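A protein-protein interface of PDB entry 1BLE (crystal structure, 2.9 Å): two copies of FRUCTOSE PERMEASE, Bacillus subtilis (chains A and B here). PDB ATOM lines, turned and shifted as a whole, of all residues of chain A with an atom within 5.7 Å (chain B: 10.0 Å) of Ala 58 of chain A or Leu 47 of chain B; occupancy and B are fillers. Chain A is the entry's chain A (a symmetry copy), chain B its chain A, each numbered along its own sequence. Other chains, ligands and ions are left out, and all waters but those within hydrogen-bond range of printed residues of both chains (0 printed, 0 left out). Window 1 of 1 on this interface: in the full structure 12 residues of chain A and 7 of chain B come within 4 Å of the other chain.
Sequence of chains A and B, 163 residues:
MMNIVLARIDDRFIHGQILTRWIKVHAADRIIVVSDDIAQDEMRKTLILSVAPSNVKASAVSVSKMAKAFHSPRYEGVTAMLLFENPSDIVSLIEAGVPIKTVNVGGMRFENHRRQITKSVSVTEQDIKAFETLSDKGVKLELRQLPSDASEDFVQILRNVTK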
ATOM      1  N   ARG A  30      31.421 -16.670  -2.680  1.00  0.00           N
ATOM      2  CA  ARG A  30      30.091 -17.154  -2.321  1.00  0.00           C
ATOM      3  C   ARG A  30      29.962 -18.195  -1.213  1.00  0.00           C
ATOM      4  O   ARG A  30      30.888 -18.959  -0.969  1.00  0.00           O
ATOM      5  CB  ARG A  30      29.440 -17.719  -3.568  1.00  0.00           C
ATOM      6  CG  ARG A  30      30.341 -18.640  -4.321  1.00  0.00           C
ATOM      7  CD  ARG A  30      29.803 -18.821  -5.730  1.00  0.00           C
ATOM      8  NE  ARG A  30      29.937 -17.635  -6.595  1.00  0.00           N
ATOM      9  CZ  ARG A  30      29.146 -17.392  -7.643  1.00  0.00           C
ATOM     10  NH1 ARG A  30      28.154 -18.242  -7.938  1.00  0.00           N
ATOM     11  NH2 ARG A  30      29.388 -16.351  -8.442  1.00  0.00           N
ATOM     12  N   ILE A  31      28.784 -18.220  -0.578  1.00  0.00           N
ATOM     13  CA  ILE A  31      28.438 -19.159   0.478  1.00  0.00           C
ATOM     14  C   ILE A  31      27.271 -19.974  -0.040  1.00  0.00           C
ATOM     15  O   ILE A  31      26.251 -19.428  -0.423  1.00  0.00           O
ATOM     16  CB  ILE A  31      27.952 -18.448   1.730  1.00  0.00           C
ATOM     17  CG1 ILE A  31      29.085 -17.697   2.348  1.00  0.00           C
ATOM     18  CG2 ILE A  31      27.489 -19.432   2.790  1.00  0.00           C
ATOM     19  CD1 ILE A  31      28.639 -17.038   3.604  1.00  0.00           C
ATOM     20  N   ILE A  32      27.399 -21.283  -0.038  1.00  0.00           N
ATOM     21  CA  ILE A  32      26.305 -22.081  -0.513  1.00  0.00           C
ATOM     22  C   ILE A  32      25.852 -23.046   0.569  1.00  0.00           C
ATOM     23  O   ILE A  32      26.669 -23.744   1.174  1.00  0.00           O
ATOM     24  CB  ILE A  32      26.722 -22.855  -1.763  1.00  0.00           C
ATOM     25  CG1 ILE A  32      27.169 -21.885  -2.842  1.00  0.00           C
ATOM     26  CG2 ILE A  32      25.582 -23.691  -2.266  1.00  0.00           C
ATOM     27  CD1 ILE A  32      28.066 -22.525  -3.863  1.00  0.00           C
ATOM     28  N   LEU A  49      19.139 -17.512   3.860  1.00  0.00           N
ATOM     29  CA  LEU A  49      19.933 -16.607   3.021  1.00  0.00           C
ATOM     30  C   LEU A  49      19.639 -15.136   3.191  1.00  0.00           C
ATOM     31  O   LEU A  49      20.120 -14.310   2.418  1.00  0.00           O
ATOM     32  CB  LEU A  49      19.681 -16.894   1.542  1.00  0.00           C
ATOM     33  CG  LEU A  49      19.450 -18.309   1.046  1.00  0.00           C
ATOM     34  CD1 LEU A  49      18.660 -18.253  -0.273  1.00  0.00           C
ATOM     35  CD2 LEU A  49      20.791 -19.009   0.898  1.00  0.00           C
ATOM     36  N   ALA A  52      22.628 -13.271   5.561  1.00  0.00           N
ATOM     37  CA  ALA A  52      24.010 -13.459   5.101  1.00  0.00           C
ATOM     38  C   ALA A  52      24.587 -12.069   4.747  1.00  0.00           C
ATOM     39  O   ALA A  52      23.831 -11.176   4.352  1.00  0.00           O
ATOM     40  CB  ALA A  52      24.024 -14.345   3.890  1.00  0.00           C
ATOM     41  N   VAL A  56      28.941 -10.517  -0.552  1.00  0.00           N
ATOM     42  CA  VAL A  56      29.047 -11.976  -0.653  1.00  0.00           C
ATOM     43  C   VAL A  56      27.761 -12.603  -1.209  1.00  0.00           C
ATOM     44  O   VAL A  56      26.670 -12.416  -0.657  1.00  0.00           O
ATOM     45  CB  VAL A  56      29.379 -12.644   0.670  1.00  0.00           C
ATOM     46  CG1 VAL A  56      30.091 -13.973   0.396  1.00  0.00           C
ATOM     47  CG2 VAL A  56      30.236 -11.734   1.509  1.00  0.00           C
ATOM     48  N   LYS A  57      27.891 -13.303  -2.327  1.00  0.00           N
ATOM     49  CA  LYS A  57      26.751 -13.941  -2.953  1.00  0.00           C
ATOM     50  C   LYS A  57      26.456 -15.201  -2.128  1.00  0.00           C
ATOM     51  O   LYS A  57      27.356 -15.827  -1.600  1.00  0.00           O
ATOM     52  CB  LYS A  57      27.054 -14.240  -4.440  1.00  0.00           C
ATOM     53  CG  LYS A  57      27.530 -12.985  -5.261  1.00  0.00           C
ATOM     54  CD  LYS A  57      28.004 -13.311  -6.704  1.00  0.00           C
ATOM     55  CE  LYS A  57      28.885 -12.192  -7.313  1.00  0.00           C
ATOM     56  NZ  LYS A  57      30.188 -11.994  -6.571  1.00  0.00           N
ATOM     57  N   ALA A  58      25.183 -15.510  -1.945  1.00  0.00           N
ATOM     58  CA  ALA A  58      24.761 -16.634  -1.148  1.00  0.00           C
ATOM     59  C   ALA A  58      23.623 -17.327  -1.823  1.00  0.00           C
ATOM     60  O   ALA A  58      22.830 -16.695  -2.469  1.00  0.00           O
ATOM     61  CB  ALA A  58      24.305 -16.141   0.148  1.00  0.00           C
ATOM     62  N   SER A  59      23.521 -18.631  -1.679  1.00  0.00           N
ATOM     63  CA  SER A  59      22.387 -19.341  -2.282  1.00  0.00           C
ATOM     64  C   SER A  59      22.232 -20.700  -1.634  1.00  0.00           C
ATOM     65  O   SER A  59      23.152 -21.189  -0.977  1.00  0.00           O
ATOM     66  CB  SER A  59      22.548 -19.484  -3.794  1.00  0.00           C
ATOM     67  OG  SER A  59      23.401 -20.575  -4.091  1.00  0.00           O
ATOM     68  N   ALA A  60      21.048 -21.278  -1.740  1.00  0.00           N
ATOM     69  CA  ALA A  60      20.823 -22.590  -1.134  1.00  0.00           C
ATOM     70  C   ALA A  60      20.387 -23.598  -2.186  1.00  0.00           C
ATOM     71  O   ALA A  60      19.383 -23.428  -2.872  1.00  0.00           O
ATOM     72  CB  ALA A  60      19.807 -22.517  -0.010  1.00  0.00           C
ATOM     73  N   ASP B  11      27.090  -8.560 -17.826  1.00  0.00           N
ATOM     74  CA  ASP B  11      27.416  -9.968 -17.519  1.00  0.00           C
ATOM     75  C   ASP B  11      27.605 -10.180 -16.048  1.00  0.00           C
ATOM     76  O   ASP B  11      27.142 -11.189 -15.551  1.00  0.00           O
ATOM     77  CB  ASP B  11      28.758 -10.354 -18.163  1.00  0.00           C
ATOM     78  CG  ASP B  11      28.615 -11.343 -19.282  1.00  0.00           C
ATOM     79  OD1 ASP B  11      27.510 -11.859 -19.513  1.00  0.00           O
ATOM     80  OD2 ASP B  11      29.623 -11.611 -19.966  1.00  0.00           O
ATOM     81  N   ARG B  12      28.325  -9.264 -15.371  1.00  0.00           N
ATOM     82  CA  ARG B  12      28.627  -9.341 -13.924  1.00  0.00           C
ATOM     83  C   ARG B  12      27.591  -8.865 -12.871  1.00  0.00           C
ATOM     84  O   ARG B  12      27.791  -9.094 -11.665  1.00  0.00           O
ATOM     85  CB  ARG B  12      30.019  -8.763 -13.636  1.00  0.00           C
ATOM     86  N   PHE B  13      26.487  -8.253 -13.345  1.00  0.00           N
ATOM     87  CA  PHE B  13      25.294  -7.756 -12.575  1.00  0.00           C
ATOM     88  C   PHE B  13      25.437  -6.678 -11.488  1.00  0.00           C
ATOM     89  O   PHE B  13      25.475  -5.469 -11.799  1.00  0.00           O
ATOM     90  CB  PHE B  13      24.449  -8.933 -12.014  1.00  0.00           C
ATOM     91  CG  PHE B  13      23.825  -9.774 -13.079  1.00  0.00           C
ATOM     92  CD1 PHE B  13      22.801  -9.268 -13.851  1.00  0.00           C
ATOM     93  CD2 PHE B  13      24.330 -11.016 -13.371  1.00  0.00           C
ATOM     94  CE1 PHE B  13      22.282  -9.982 -14.897  1.00  0.00           C
ATOM     95  CE2 PHE B  13      23.820 -11.741 -14.412  1.00  0.00           C
ATOM     96  CZ  PHE B  13      22.790 -11.221 -15.187  1.00  0.00           C
ATOM     97  N   ILE B  14      25.374  -7.141 -10.229  1.00  0.00           N
ATOM     98  CA  ILE B  14      25.511  -6.308  -9.024  1.00  0.00           C
ATOM     99  C   ILE B  14      26.962  -6.415  -8.523  1.00  0.00           C
ATOM    100  O   ILE B  14      27.243  -7.085  -7.508  1.00  0.00           O
ATOM    101  CB  ILE B  14      24.562  -6.773  -7.911  1.00  0.00           C
ATOM    102  CG1 ILE B  14      23.287  -7.390  -8.518  1.00  0.00           C
ATOM    103  CG2 ILE B  14      24.255  -5.608  -7.006  1.00  0.00           C
ATOM    104  CD1 ILE B  14      22.028  -6.576  -8.385  1.00  0.00           C
ATOM    105  N   HIS B  15      27.871  -5.811  -9.297  1.00  0.00           N
ATOM    106  CA  HIS B  15      29.301  -5.776  -9.020  1.00  0.00           C
ATOM    107  C   HIS B  15      29.722  -4.341  -8.655  1.00  0.00           C
ATOM    108  O   HIS B  15      29.291  -3.376  -9.301  1.00  0.00           O
ATOM    109  CB  HIS B  15      30.086  -6.261 -10.259  1.00  0.00           C
ATOM    110  CG  HIS B  15      31.562  -6.004 -10.186  1.00  0.00           C
ATOM    111  ND1 HIS B  15      32.099  -4.731 -10.066  1.00  0.00           N
ATOM    112  CD2 HIS B  15      32.622  -6.848 -10.188  1.00  0.00           C
ATOM    113  CE1 HIS B  15      33.410  -4.807  -9.991  1.00  0.00           C
ATOM    114  NE2 HIS B  15      33.759  -6.086 -10.064  1.00  0.00           N
ATOM    115  N   VAL B  33      16.314  -7.986 -12.998  1.00  0.00           N
ATOM    116  CA  VAL B  33      17.199  -8.724 -13.918  1.00  0.00           C
ATOM    117  C   VAL B  33      16.262  -9.504 -14.834  1.00  0.00           C
ATOM    118  O   VAL B  33      15.368 -10.227 -14.371  1.00  0.00           O
ATOM    119  CB  VAL B  33      18.175  -9.680 -13.160  1.00  0.00           C
ATOM    120  CG1 VAL B  33      18.859 -10.624 -14.110  1.00  0.00           C
ATOM    121  CG2 VAL B  33      19.226  -8.875 -12.493  1.00  0.00           C
ATOM    122  N   ILE B  38      18.582 -17.267 -15.963  1.00  0.00           N
ATOM    123  CA  ILE B  38      18.739 -16.861 -14.573  1.00  0.00           C
ATOM    124  C   ILE B  38      17.442 -17.010 -13.750  1.00  0.00           C
ATOM    125  O   ILE B  38      17.479 -17.216 -12.547  1.00  0.00           O
ATOM    126  CB  ILE B  38      19.226 -15.373 -14.537  1.00  0.00           C
ATOM    127  CG1 ILE B  38      20.677 -15.259 -15.009  1.00  0.00           C
ATOM    128  CG2 ILE B  38      19.072 -14.767 -13.177  1.00  0.00           C
ATOM    129  CD1 ILE B  38      21.110 -13.855 -15.390  1.00  0.00           C
ATOM    130  N   ASP B  41      17.027 -20.773 -12.836  1.00  0.00           N
ATOM    131  CA  ASP B  41      18.165 -21.370 -12.165  1.00  0.00           C
ATOM    132  C   ASP B  41      18.223 -20.893 -10.752  1.00  0.00           C
ATOM    133  O   ASP B  41      18.754 -19.833 -10.476  1.00  0.00           O
ATOM    134  CB  ASP B  41      19.461 -21.026 -12.896  1.00  0.00           C
ATOM    135  CG  ASP B  41      20.632 -21.946 -12.508  1.00  0.00           C
ATOM    136  OD1 ASP B  41      21.051 -21.979 -11.325  1.00  0.00           O
ATOM    137  OD2 ASP B  41      21.145 -22.640 -13.418  1.00  0.00           O
ATOM    138  N   GLU B  42      17.707 -21.722  -9.855  1.00  0.00           N
ATOM    139  CA  GLU B  42      17.659 -21.436  -8.415  1.00  0.00           C
ATOM    140  C   GLU B  42      18.987 -20.980  -7.765  1.00  0.00           C
ATOM    141  O   GLU B  42      19.007 -20.085  -6.926  1.00  0.00           O
ATOM    142  CB  GLU B  42      17.063 -22.637  -7.664  1.00  0.00           C
ATOM    143  N   MET B  43      20.090 -21.573  -8.169  1.00  0.00           N
ATOM    144  CA  MET B  43      21.389 -21.202  -7.633  1.00  0.00           C
ATOM    145  C   MET B  43      21.894 -19.862  -8.163  1.00  0.00           C
ATOM    146  O   MET B  43      22.833 -19.282  -7.617  1.00  0.00           O
ATOM    147  CB  MET B  43      22.410 -22.296  -7.986  1.00  0.00           C
ATOM    148  CG  MET B  43      23.846 -21.866  -8.022  1.00  0.00           C
ATOM    149  SD  MET B  43      24.854 -22.979  -7.150  1.00  0.00           S
ATOM    150  CE  MET B  43      25.979 -21.846  -6.306  1.00  0.00           C
ATOM    151  N   ARG B  44      21.277 -19.352  -9.213  1.00  0.00           N
ATOM    152  CA  ARG B  44      21.742 -18.114  -9.796  1.00  0.00           C
ATOM    153  C   ARG B  44      20.788 -16.937  -9.557  1.00  0.00           C
ATOM    154  O   ARG B  44      21.234 -15.792  -9.490  1.00  0.00           O
ATOM    155  CB  ARG B  44      22.005 -18.376 -11.275  1.00  0.00           C
ATOM    156  CG  ARG B  44      23.177 -17.660 -11.881  1.00  0.00           C
ATOM    157  CD  ARG B  44      23.461 -18.183 -13.306  1.00  0.00           C
ATOM    158  NE  ARG B  44      23.938 -17.113 -14.197  1.00  0.00           N
ATOM    159  CZ  ARG B  44      23.588 -16.992 -15.478  1.00  0.00           C
ATOM    160  NH1 ARG B  44      22.767 -17.877 -16.044  1.00  0.00           N
ATOM    161  NH2 ARG B  44      23.989 -15.931 -16.163  1.00  0.00           N
ATOM    162  N   LYS B  45      19.481 -17.194  -9.431  1.00  0.00           N
ATOM    163  CA  LYS B  45      18.540 -16.095  -9.176  1.00  0.00           C
ATOM    164  C   LYS B  45      18.909 -15.505  -7.803  1.00  0.00           C
ATOM    165  O   LYS B  45      19.260 -14.326  -7.701  1.00  0.00           O
ATOM    166  CB  LYS B  45      17.069 -16.549  -9.193  1.00  0.00           C
ATOM    167  N   THR B  46      18.928 -16.352  -6.773  1.00  0.00           N
ATOM    168  CA  THR B  46      19.271 -15.935  -5.407  1.00  0.00           C
ATOM    169  C   THR B  46      20.596 -15.204  -5.401  1.00  0.00           C
ATOM    170  O   THR B  46      20.656 -14.016  -5.154  1.00  0.00           O
ATOM    171  CB  THR B  46      19.446 -17.139  -4.505  1.00  0.00           C
ATOM    172  OG1 THR B  46      18.223 -17.880  -4.445  1.00  0.00           O
ATOM    173  CG2 THR B  46      19.821 -16.694  -3.132  1.00  0.00           C
ATOM    174  N   LEU B  47      21.641 -15.941  -5.756  1.00  0.00           N
ATOM    175  CA  LEU B  47      23.016 -15.452  -5.842  1.00  0.00           C
ATOM    176  C   LEU B  47      23.191 -14.128  -6.597  1.00  0.00           C
ATOM    177  O   LEU B  47      24.138 -13.408  -6.333  1.00  0.00           O
ATOM    178  CB  LEU B  47      23.924 -16.536  -6.441  1.00  0.00           C
ATOM    179  N   ILE B  48      22.306 -13.782  -7.522  1.00  0.00           N
ATOM    180  CA  ILE B  48      22.466 -12.494  -8.195  1.00  0.00           C
ATOM    181  C   ILE B  48      21.868 -11.387  -7.319  1.00  0.00           C
ATOM    182  O   ILE B  48      22.562 -10.456  -6.960  1.00  0.00           O
ATOM    183  CB  ILE B  48      21.835 -12.467  -9.630  1.00  0.00           C
ATOM    184  N   LEU B  49      20.627 -11.584  -6.880  1.00  0.00           N
ATOM    185  CA  LEU B  49      19.868 -10.619  -6.075  1.00  0.00           C
ATOM    186  C   LEU B  49      20.289 -10.503  -4.631  1.00  0.00           C
ATOM    187  O   LEU B  49      19.612  -9.858  -3.832  1.00  0.00           O
ATOM    188  CB  LEU B  49      18.392 -11.010  -6.027  1.00  0.00           C
ATOM    189  CG  LEU B  49      17.706 -11.634  -7.229  1.00  0.00           C
ATOM    190  CD1 LEU B  49      16.491 -12.443  -6.747  1.00  0.00           C
ATOM    191  CD2 LEU B  49      17.329 -10.536  -8.211  1.00  0.00           C
ATOM    192  N   SER B  50      21.324 -11.224  -4.248  1.00  0.00           N
ATOM    193  CA  SER B  50      21.766 -11.170  -2.859  1.00  0.00           C
ATOM    194  C   SER B  50      22.890 -10.153  -2.570  1.00  0.00           C
ATOM    195  O   SER B  50      23.332 -10.023  -1.441  1.00  0.00           O
ATOM    196  CB  SER B  50      22.150 -12.578  -2.364  1.00  0.00           C
ATOM    197  OG  SER B  50      23.187 -13.160  -3.138  1.00  0.00           O
ATOM    198  N   VAL B  51      23.360  -9.448  -3.583  1.00  0.00           N
ATOM    199  CA  VAL B  51      24.398  -8.492  -3.359  1.00  0.00           C
ATOM    200  C   VAL B  51      23.948  -7.159  -3.873  1.00  0.00           C
ATOM    201  O   VAL B  51      24.773  -6.294  -4.162  1.00  0.00           O
ATOM    202  CB  VAL B  51      25.679  -8.919  -4.006  1.00  0.00           C
ATOM    203  CG1 VAL B  51      26.428  -9.802  -3.067  1.00  0.00           C
ATOM    204  CG2 VAL B  51      25.389  -9.626  -5.329  1.00  0.00           C
ATOM    205  N   ALA B  52      22.631  -7.014  -4.026  1.00  0.00           N
ATOM    206  CA  ALA B  52      22.022  -5.756  -4.476  1.00  0.00           C
ATOM    207  C   ALA B  52      21.835  -4.847  -3.239  1.00  0.00           C
ATOM    208  O   ALA B  52      21.654  -5.357  -2.128  1.00  0.00           O
ATOM    209  CB  ALA B  52      20.693  -6.037  -5.113  1.00  0.00           C
ATOM    210  N   ALA B  60      14.360 -11.021  -9.977  1.00  0.00           N
ATOM    211  CA  ALA B  60      14.774 -11.557 -11.274  1.00  0.00           C
ATOM    212  C   ALA B  60      13.624 -12.296 -11.940  1.00  0.00           C
ATOM    213  O   ALA B  60      13.067 -13.250 -11.404  1.00  0.00           O
ATOM    214  CB  ALA B  60      15.985 -12.460 -11.141  1.00  0.00           C
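Of the 10 printed residues of chain A, 6 touch a printed residue of chain B.
Hydrophobic or aromatic side chains of chain A that line the printed part of chain B: Ile 32 and Leu 49.
Among the printed residues, no Asp or Glu carboxylate lies within 4 Å of a Lys or Arg side-chain nitrogen of the other chain.
No residue of chain B comes within 4 Å of Ile 31 of chain A.
Of the printed residues of chain B, Ile 32 of chain A touches Met 43.
Ala 58 of chain A touches three residues of chain B.
Ser 59 of chain A touches two residues of chain B.
Asp 11 of chain B touches none of the printed residues of chain A.
Glu 42 of chain B touches none of the printed residues of chain A.
Of the printed residues of chain A, Thr 46 of chain B touches Leu 49, Ala 58 and Ser 59.
Of chain A, only Lys 57 (3.6 Å) and Ala 58 (3.6 Å) come within 4 Å of Leu 47 of chain B.
The nearest residue of chain B that does not touch Ala 58 of chain A is Met 43 of chain B (5.8 Å).
The nearest residue of chain A that does not touch Leu 47 of chain B is Ser 59 of chain A (4.2 Å).
3 positions are printed for both chains.
The backbone NH (N) of Ala 58 of chain A lies within hydrogen-bond range of the side-chain hydroxyl (OG) of Ser 50 of chain B (3.3 Å).
Among the printed residues, merely in contact across the chains: Ile 32 of chain A with Met 43 of chain B, Leu 49 of chain A with Thr 46 of chain B, Val 56 of chain A with Val 51 of chain B, Lys 57 of chain A with Leu 47 of chain B, Lys 57 of chain A with Ser 50 of chain B, Lys 57 of chain A with Val 51 of chain B, Ala 58 of chain A with Thr 46 of chain B, Ala 58 of chain A with Leu 47 of chain B, Ser 59 of chain A with Met 43 of chain B and Ser 59 of chain A with Thr 46 of chain B.
The side-chain carboxylate (OD1) of Asp 41 of chain B lies close to the backbone NH (N) of Met 43 of chain B (3.3 Å).
The side-chain hydroxyl (OG1) of Thr 46 of chain B lies within hydrogen-bond range of the backbone carbonyl oxygen (O) of Glu 42 of chain B (3.4 Å).
The backbone carbonyl oxygen (O) of Thr 46 of chain B sits at hydrogen-bond distance from the side-chain hydroxyl (OG) of Ser 50 of chain B (3.3 Å).
The backbone carbonyl oxygen of Leu 47 of chain B is in hydrogen-bond range of the side-chain hydroxyl of Ser 50 of chain B (3.3 Å).
The backbone NH (N) of Ile 31 of chain A lies within hydrogen-bond range of the backbone carbonyl oxygen (O) of Lys 57 of chain A, at 3.0 Å.
The backbone carbonyl oxygen (O) of Ile 31 of chain A lies within hydrogen-bond range of the backbone NH (N) of Ser 59 of chain A, 3.1 Å away.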
